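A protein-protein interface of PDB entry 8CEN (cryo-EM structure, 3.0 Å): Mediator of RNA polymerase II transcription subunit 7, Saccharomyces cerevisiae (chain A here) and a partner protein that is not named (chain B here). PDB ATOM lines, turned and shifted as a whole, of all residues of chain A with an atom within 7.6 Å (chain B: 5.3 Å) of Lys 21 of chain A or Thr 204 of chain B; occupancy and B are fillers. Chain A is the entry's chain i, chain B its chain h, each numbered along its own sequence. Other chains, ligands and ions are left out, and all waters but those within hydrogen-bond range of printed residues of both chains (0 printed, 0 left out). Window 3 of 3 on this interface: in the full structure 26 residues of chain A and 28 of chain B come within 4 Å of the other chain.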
ATOM      1  N   PRO A  17     -18.207  29.557 -17.848  1.00  0.00           N
ATOM      2  CA  PRO A  17     -18.523  28.147 -17.614  1.00  0.00           C
ATOM      3  C   PRO A  17     -17.345  27.249 -17.944  1.00  0.00           C
ATOM      4  O   PRO A  17     -16.563  27.537 -18.868  1.00  0.00           O
ATOM      5  CB  PRO A  17     -19.706  27.887 -18.566  1.00  0.00           C
ATOM      6  CG  PRO A  17     -20.275  29.219 -18.848  1.00  0.00           C
ATOM      7  CD  PRO A  17     -19.118  30.158 -18.839  1.00  0.00           C
ATOM      8  N   PRO A  18     -17.207  26.113 -17.247  1.00  0.00           N
ATOM      9  CA  PRO A  18     -16.089  25.193 -17.530  1.00  0.00           C
ATOM     10  C   PRO A  18     -16.109  24.638 -18.939  1.00  0.00           C
ATOM     11  O   PRO A  18     -15.070  24.172 -19.425  1.00  0.00           O
ATOM     12  CB  PRO A  18     -16.285  24.080 -16.491  1.00  0.00           C
ATOM     13  CG  PRO A  18     -17.742  24.129 -16.167  1.00  0.00           C
ATOM     14  CD  PRO A  18     -18.113  25.578 -16.218  1.00  0.00           C
ATOM     15  N   TYR A  19     -17.251  24.745 -19.625  1.00  0.00           N
ATOM     16  CA  TYR A  19     -17.395  24.339 -21.017  1.00  0.00           C
ATOM     17  C   TYR A  19     -16.391  25.046 -21.921  1.00  0.00           C
ATOM     18  O   TYR A  19     -16.027  24.509 -22.976  1.00  0.00           O
ATOM     19  CB  TYR A  19     -18.824  24.644 -21.471  1.00  0.00           C
ATOM     20  CG  TYR A  19     -19.899  23.950 -20.654  1.00  0.00           C
ATOM     21  CD1 TYR A  19     -19.647  22.749 -19.998  1.00  0.00           C
ATOM     22  CD2 TYR A  19     -21.146  24.537 -20.482  1.00  0.00           C
ATOM     23  CE1 TYR A  19     -20.620  22.136 -19.235  1.00  0.00           C
ATOM     24  CE2 TYR A  19     -22.120  23.931 -19.715  1.00  0.00           C
ATOM     25  CZ  TYR A  19     -21.854  22.728 -19.100  1.00  0.00           C
ATOM     26  OH  TYR A  19     -22.823  22.117 -18.338  1.00  0.00           O
ATOM     27  N   VAL A  20     -15.911  26.232 -21.504  1.00  0.00           N
ATOM     28  CA  VAL A  20     -14.893  26.977 -22.250  1.00  0.00           C
ATOM     29  C   VAL A  20     -13.645  26.133 -22.508  1.00  0.00           C
ATOM     30  O   VAL A  20     -13.004  26.275 -23.558  1.00  0.00           O
ATOM     31  CB  VAL A  20     -14.556  28.291 -21.504  1.00  0.00           C
ATOM     32  CG1 VAL A  20     -13.418  29.053 -22.170  1.00  0.00           C
ATOM     33  CG2 VAL A  20     -15.764  29.193 -21.455  1.00  0.00           C
ATOM     34  N   LYS A  21     -13.317  25.191 -21.609  1.00  0.00           N
ATOM     35  CA  LYS A  21     -12.101  24.410 -21.831  1.00  0.00           C
ATOM     36  C   LYS A  21     -12.214  23.441 -23.003  1.00  0.00           C
ATOM     37  O   LYS A  21     -11.185  22.927 -23.452  1.00  0.00           O
ATOM     38  CB  LYS A  21     -11.708  23.615 -20.583  1.00  0.00           C
ATOM     39  CG  LYS A  21     -12.594  22.423 -20.279  1.00  0.00           C
ATOM     40  CD  LYS A  21     -12.051  21.622 -19.110  1.00  0.00           C
ATOM     41  CE  LYS A  21     -12.254  20.132 -19.324  1.00  0.00           C
ATOM     42  NZ  LYS A  21     -11.792  19.335 -18.156  1.00  0.00           N
ATOM     43  N   PHE A  22     -13.419  23.179 -23.514  1.00  0.00           N
ATOM     44  CA  PHE A  22     -13.566  22.234 -24.613  1.00  0.00           C
ATOM     45  C   PHE A  22     -13.393  22.859 -25.991  1.00  0.00           C
ATOM     46  O   PHE A  22     -13.301  22.119 -26.977  1.00  0.00           O
ATOM     47  CB  PHE A  22     -14.934  21.547 -24.548  1.00  0.00           C
ATOM     48  CG  PHE A  22     -15.094  20.626 -23.377  1.00  0.00           C
ATOM     49  CD1 PHE A  22     -14.339  19.468 -23.284  1.00  0.00           C
ATOM     50  CD2 PHE A  22     -16.006  20.909 -22.373  1.00  0.00           C
ATOM     51  CE1 PHE A  22     -14.484  18.614 -22.209  1.00  0.00           C
ATOM     52  CE2 PHE A  22     -16.157  20.058 -21.296  1.00  0.00           C
ATOM     53  CZ  PHE A  22     -15.395  18.909 -21.215  1.00  0.00           C
ATOM     54  N   PHE A  23     -13.342  24.187 -26.094  1.00  0.00           N
ATOM     55  CA  PHE A  23     -13.433  24.855 -27.394  1.00  0.00           C
ATOM     56  C   PHE A  23     -12.040  25.231 -27.890  1.00  0.00           C
ATOM     57  O   PHE A  23     -11.627  26.391 -27.879  1.00  0.00           O
ATOM     58  CB  PHE A  23     -14.347  26.068 -27.298  1.00  0.00           C
ATOM     59  CG  PHE A  23     -15.794  25.711 -27.200  1.00  0.00           C
ATOM     60  CD1 PHE A  23     -16.371  25.451 -25.971  1.00  0.00           C
ATOM     61  CD2 PHE A  23     -16.570  25.601 -28.338  1.00  0.00           C
ATOM     62  CE1 PHE A  23     -17.699  25.107 -25.875  1.00  0.00           C
ATOM     63  CE2 PHE A  23     -17.897  25.255 -28.248  1.00  0.00           C
ATOM     64  CZ  PHE A  23     -18.463  25.012 -27.014  1.00  0.00           C
ATOM     65  N   THR A  24     -11.322  24.222 -28.369  1.00  0.00           N
ATOM     66  CA  THR A  24      -9.982  24.387 -28.906  1.00  0.00           C
ATOM     67  C   THR A  24     -10.011  24.288 -30.427  1.00  0.00           C
ATOM     68  O   THR A  24     -11.036  23.962 -31.036  1.00  0.00           O
ATOM     69  CB  THR A  24      -9.030  23.338 -28.326  1.00  0.00           C
ATOM     70  OG1 THR A  24      -9.408  22.040 -28.797  1.00  0.00           O
ATOM     71  CG2 THR A  24      -9.091  23.352 -26.809  1.00  0.00           C
ATOM     72  N   ASN A  27     -10.610  20.647 -31.456  1.00  0.00           N
ATOM     73  CA  ASN A  27     -12.019  20.293 -31.317  1.00  0.00           C
ATOM     74  C   ASN A  27     -12.862  20.932 -32.415  1.00  0.00           C
ATOM     75  O   ASN A  27     -13.767  20.290 -32.959  1.00  0.00           O
ATOM     76  CB  ASN A  27     -12.530  20.697 -29.935  1.00  0.00           C
ATOM     77  CG  ASN A  27     -11.980  19.813 -28.831  1.00  0.00           C
ATOM     78  OD1 ASN A  27     -12.571  18.789 -28.489  1.00  0.00           O
ATOM     79  ND2 ASN A  27     -10.842  20.204 -28.271  1.00  0.00           N
ATOM     80  N   ILE A  58     -24.102  12.685 -23.140  1.00  0.00           N
ATOM     81  CA  ILE A  58     -22.807  13.083 -23.675  1.00  0.00           C
ATOM     82  C   ILE A  58     -22.008  11.841 -24.043  1.00  0.00           C
ATOM     83  O   ILE A  58     -21.800  10.946 -23.214  1.00  0.00           O
ATOM     84  CB  ILE A  58     -22.050  13.952 -22.661  1.00  0.00           C
ATOM     85  CG1 ILE A  58     -22.863  15.203 -22.317  1.00  0.00           C
ATOM     86  CG2 ILE A  58     -20.684  14.337 -23.203  1.00  0.00           C
ATOM     87  CD1 ILE A  58     -23.134  16.103 -23.500  1.00  0.00           C
ATOM     88  N   CYS A  60     -18.952  12.215 -26.213  1.00  0.00           N
ATOM     89  CA  CYS A  60     -17.563  12.595 -26.434  1.00  0.00           C
ATOM     90  C   CYS A  60     -17.395  14.061 -26.055  1.00  0.00           C
ATOM     91  O   CYS A  60     -18.331  14.714 -25.586  1.00  0.00           O
ATOM     92  CB  CYS A  60     -17.143  12.340 -27.885  1.00  0.00           C
ATOM     93  SG  CYS A  60     -17.809  13.526 -29.068  1.00  0.00           S
ATOM     94  N   ALA A  61     -16.180  14.575 -26.262  1.00  0.00           N
ATOM     95  CA  ALA A  61     -15.888  15.965 -25.933  1.00  0.00           C
ATOM     96  C   ALA A  61     -16.496  16.940 -26.933  1.00  0.00           C
ATOM     97  O   ALA A  61     -16.653  18.121 -26.608  1.00  0.00           O
ATOM     98  CB  ALA A  61     -14.377  16.181 -25.852  1.00  0.00           C
ATOM     99  N   TYR A  64     -20.173  19.038 -26.452  1.00  0.00           N
ATOM    100  CA  TYR A  64     -20.291  20.371 -25.883  1.00  0.00           C
ATOM    101  C   TYR A  64     -20.128  21.464 -26.928  1.00  0.00           C
ATOM    102  O   TYR A  64     -20.476  22.616 -26.653  1.00  0.00           O
ATOM    103  CB  TYR A  64     -19.264  20.565 -24.767  1.00  0.00           C
ATOM    104  CG  TYR A  64     -19.531  19.716 -23.546  1.00  0.00           C
ATOM    105  CD1 TYR A  64     -19.055  18.412 -23.466  1.00  0.00           C
ATOM    106  CD2 TYR A  64     -20.271  20.208 -22.481  1.00  0.00           C
ATOM    107  CE1 TYR A  64     -19.300  17.631 -22.355  1.00  0.00           C
ATOM    108  CE2 TYR A  64     -20.522  19.431 -21.367  1.00  0.00           C
ATOM    109  CZ  TYR A  64     -20.034  18.146 -21.309  1.00  0.00           C
ATOM    110  OH  TYR A  64     -20.280  17.370 -20.201  1.00  0.00           O
ATOM    111  N   LEU A  65     -19.622  21.128 -28.113  1.00  0.00           N
ATOM    112  CA  LEU A  65     -19.492  22.079 -29.207  1.00  0.00           C
ATOM    113  C   LEU A  65     -20.778  22.225 -30.008  1.00  0.00           C
ATOM    114  O   LEU A  65     -20.864  23.114 -30.863  1.00  0.00           O
ATOM    115  CB  LEU A  65     -18.350  21.651 -30.136  1.00  0.00           C
ATOM    116  CG  LEU A  65     -16.941  22.187 -29.863  1.00  0.00           C
ATOM    117  CD1 LEU A  65     -16.349  21.609 -28.584  1.00  0.00           C
ATOM    118  CD2 LEU A  65     -16.037  21.891 -31.042  1.00  0.00           C
ATOM    119  N   SER B 200     -18.368  22.450 -11.385  1.00  0.00           N
ATOM    120  CA  SER B 200     -17.739  22.335 -12.698  1.00  0.00           C
ATOM    121  C   SER B 200     -17.251  20.920 -12.993  1.00  0.00           C
ATOM    122  O   SER B 200     -17.189  20.523 -14.162  1.00  0.00           O
ATOM    123  CB  SER B 200     -16.574  23.318 -12.798  1.00  0.00           C
ATOM    124  OG  SER B 200     -15.659  23.135 -11.733  1.00  0.00           O
ATOM    125  N   LYS B 201     -16.891  20.155 -11.961  1.00  0.00           N
ATOM    126  CA  LYS B 201     -16.418  18.792 -12.185  1.00  0.00           C
ATOM    127  C   LYS B 201     -17.542  17.879 -12.667  1.00  0.00           C
ATOM    128  O   LYS B 201     -17.338  17.069 -13.578  1.00  0.00           O
ATOM    129  CB  LYS B 201     -15.783  18.241 -10.909  1.00  0.00           C
ATOM    130  CG  LYS B 201     -15.221  16.835 -11.056  1.00  0.00           C
ATOM    131  CD  LYS B 201     -14.084  16.797 -12.065  1.00  0.00           C
ATOM    132  CE  LYS B 201     -12.850  17.513 -11.543  1.00  0.00           C
ATOM    133  NZ  LYS B 201     -11.716  17.423 -12.503  1.00  0.00           N
ATOM    134  N   GLU B 202     -18.734  18.000 -12.078  1.00  0.00           N
ATOM    135  CA  GLU B 202     -19.840  17.128 -12.467  1.00  0.00           C
ATOM    136  C   GLU B 202     -20.410  17.496 -13.832  1.00  0.00           C
ATOM    137  O   GLU B 202     -20.930  16.625 -14.537  1.00  0.00           O
ATOM    138  CB  GLU B 202     -20.945  17.160 -11.407  1.00  0.00           C
ATOM    139  CG  GLU B 202     -20.571  16.545 -10.056  1.00  0.00           C
ATOM    140  CD  GLU B 202     -19.808  17.491  -9.149  1.00  0.00           C
ATOM    141  OE1 GLU B 202     -19.614  18.661  -9.533  1.00  0.00           O
ATOM    142  OE2 GLU B 202     -19.404  17.061  -8.048  1.00  0.00           O
ATOM    143  N   LEU B 203     -20.330  18.770 -14.222  1.00  0.00           N
ATOM    144  CA  LEU B 203     -20.878  19.192 -15.507  1.00  0.00           C
ATOM    145  C   LEU B 203     -19.990  18.797 -16.679  1.00  0.00           C
ATOM    146  O   LEU B 203     -20.469  18.750 -17.817  1.00  0.00           O
ATOM    147  CB  LEU B 203     -21.086  20.705 -15.519  1.00  0.00           C
ATOM    148  CG  LEU B 203     -22.056  21.253 -14.478  1.00  0.00           C
ATOM    149  CD1 LEU B 203     -22.189  22.752 -14.621  1.00  0.00           C
ATOM    150  CD2 LEU B 203     -23.397  20.577 -14.599  1.00  0.00           C
ATOM    151  N   THR B 204     -18.718  18.513 -16.424  1.00  0.00           N
ATOM    152  CA  THR B 204     -17.712  18.308 -17.454  1.00  0.00           C
ATOM    153  C   THR B 204     -17.580  16.833 -17.844  1.00  0.00           C
ATOM    154  O   THR B 204     -17.062  16.535 -18.928  1.00  0.00           O
ATOM    155  CB  THR B 204     -16.387  18.923 -16.928  1.00  0.00           C
ATOM    156  OG1 THR B 204     -16.468  20.352 -17.025  1.00  0.00           O
ATOM    157  CG2 THR B 204     -15.114  18.472 -17.648  1.00  0.00           C
ATOM    158  N   ARG B 205     -18.211  15.936 -17.080  1.00  0.00           N
ATOM    159  CA  ARG B 205     -17.905  14.507 -17.092  1.00  0.00           C
ATOM    160  C   ARG B 205     -18.107  13.864 -18.463  1.00  0.00           C
ATOM    161  O   ARG B 205     -19.139  14.058 -19.112  1.00  0.00           O
ATOM    162  CB  ARG B 205     -18.782  13.790 -16.064  1.00  0.00           C
ATOM    163  CG  ARG B 205     -18.492  14.147 -14.615  1.00  0.00           C
ATOM    164  CD  ARG B 205     -19.393  13.358 -13.676  1.00  0.00           C
ATOM    165  NE  ARG B 205     -19.213  13.737 -12.280  1.00  0.00           N
ATOM    166  CZ  ARG B 205     -18.328  13.189 -11.459  1.00  0.00           C
ATOM    167  NH1 ARG B 205     -17.503  12.239 -11.865  1.00  0.00           N
ATOM    168  NH2 ARG B 205     -18.269  13.606 -10.197  1.00  0.00           N
ATOM    169  N   ILE B 206     -17.110  13.097 -18.890  1.00  0.00           N
ATOM    170  CA  ILE B 206     -17.143  12.347 -20.139  1.00  0.00           C
ATOM    171  C   ILE B 206     -17.096  10.867 -19.788  1.00  0.00           C
ATOM    172  O   ILE B 206     -16.270  10.466 -18.967  1.00  0.00           O
ATOM    173  CB  ILE B 206     -15.972  12.708 -21.074  1.00  0.00           C
ATOM    174  CG1 ILE B 206     -15.787  14.222 -21.164  1.00  0.00           C
ATOM    175  CG2 ILE B 206     -16.174  12.115 -22.461  1.00  0.00           C
ATOM    176  CD1 ILE B 206     -16.979  14.932 -21.757  1.00  0.00           C
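The backbone carbonyl oxygen (O) of Leu 203 of chain B lies within hydrogen-bond range of the side-chain hydroxyl (OH) of Tyr 64 of chain A, at 2.8 Å.
O of Ser 200 of chain B is in hydrogen-bond range of OG1 of Thr 204 of chain B (3.0 Å).
ND2 of Asn 27 of chain A lies close to O of Phe 22 of chain A (3.4 Å).
Ser 200 of chain B touches Pro 18 of chain A (CB to CG, 3.7 Å).
Thr 204 of chain B touches Pro 18 of chain A.
CB of Leu 203 of chain B touches OH of Tyr 19 of chain A, at 3.6 Å.
Lys 21 of chain A touches Thr 204 of chain B.
Phe 22 of chain A touches Thr 204 of chain B.
Thr 204 of chain B touches Tyr 64 of chain A.
OH of Tyr 64 of chain A touches O of Arg 205 of chain B, at 3.7 Å.
Tyr 64 of chain A touches Ile 206 of chain B.
Of the printed residues of chain B, Lys 21 of chain A touches Thr 204.
Thr 204 of chain B touches just these residues of chain A: Pro 18, Lys 21, Phe 22 and Tyr 64.
Of the printed residues of chain A, Ser 200 of chain B touches Pro 18 (3.7 Å).
Printed residues of chain B within 4 Å of Phe 22 of chain A: Thr 204 (3.6 Å).
Of the printed residues of chain A, Leu 203 of chain B touches Tyr 19 (3.6 Å) and Tyr 64 (2.8 Å).
Pro 17 of chain A touches none of the printed residues of chain B.
Ala 61 of chain A touches none of the printed residues of chain B.
The nearest printed residue of chain B that does not touch Lys 21 of chain A is Lys 201 of chain B (6.0 Å).
The nearest residue of chain A that does not touch Thr 204 of chain B is Tyr 19 of chain A (5.0 Å).
The nearest printed residue of chain B that does not touch Tyr 19 of chain A is Thr 204 of chain B (5.0 Å).
Of the 7 printed residues of chain B, 5 touch a printed residue of chain A.
Hydrophobic or aromatic side chains of chain B that line the printed part of chain A: Leu 203 and Ile 206.
Of the 14 printed residues of chain A, 5 touch a printed residue of chain B.
Printed residues of chain A that touch a printed residue of chain B: Pro 18, Tyr 19, Lys 21, Phe 22 and Tyr 64.
Hydrophobic or aromatic side chains of chain A that line the printed part of chain B: Pro 18, Tyr 19, Phe 22 and Tyr 64.
Among the printed residues, no Asp or Glu carboxylate lies within 4 Å of a Lys or Arg side-chain nitrogen of the other chain.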
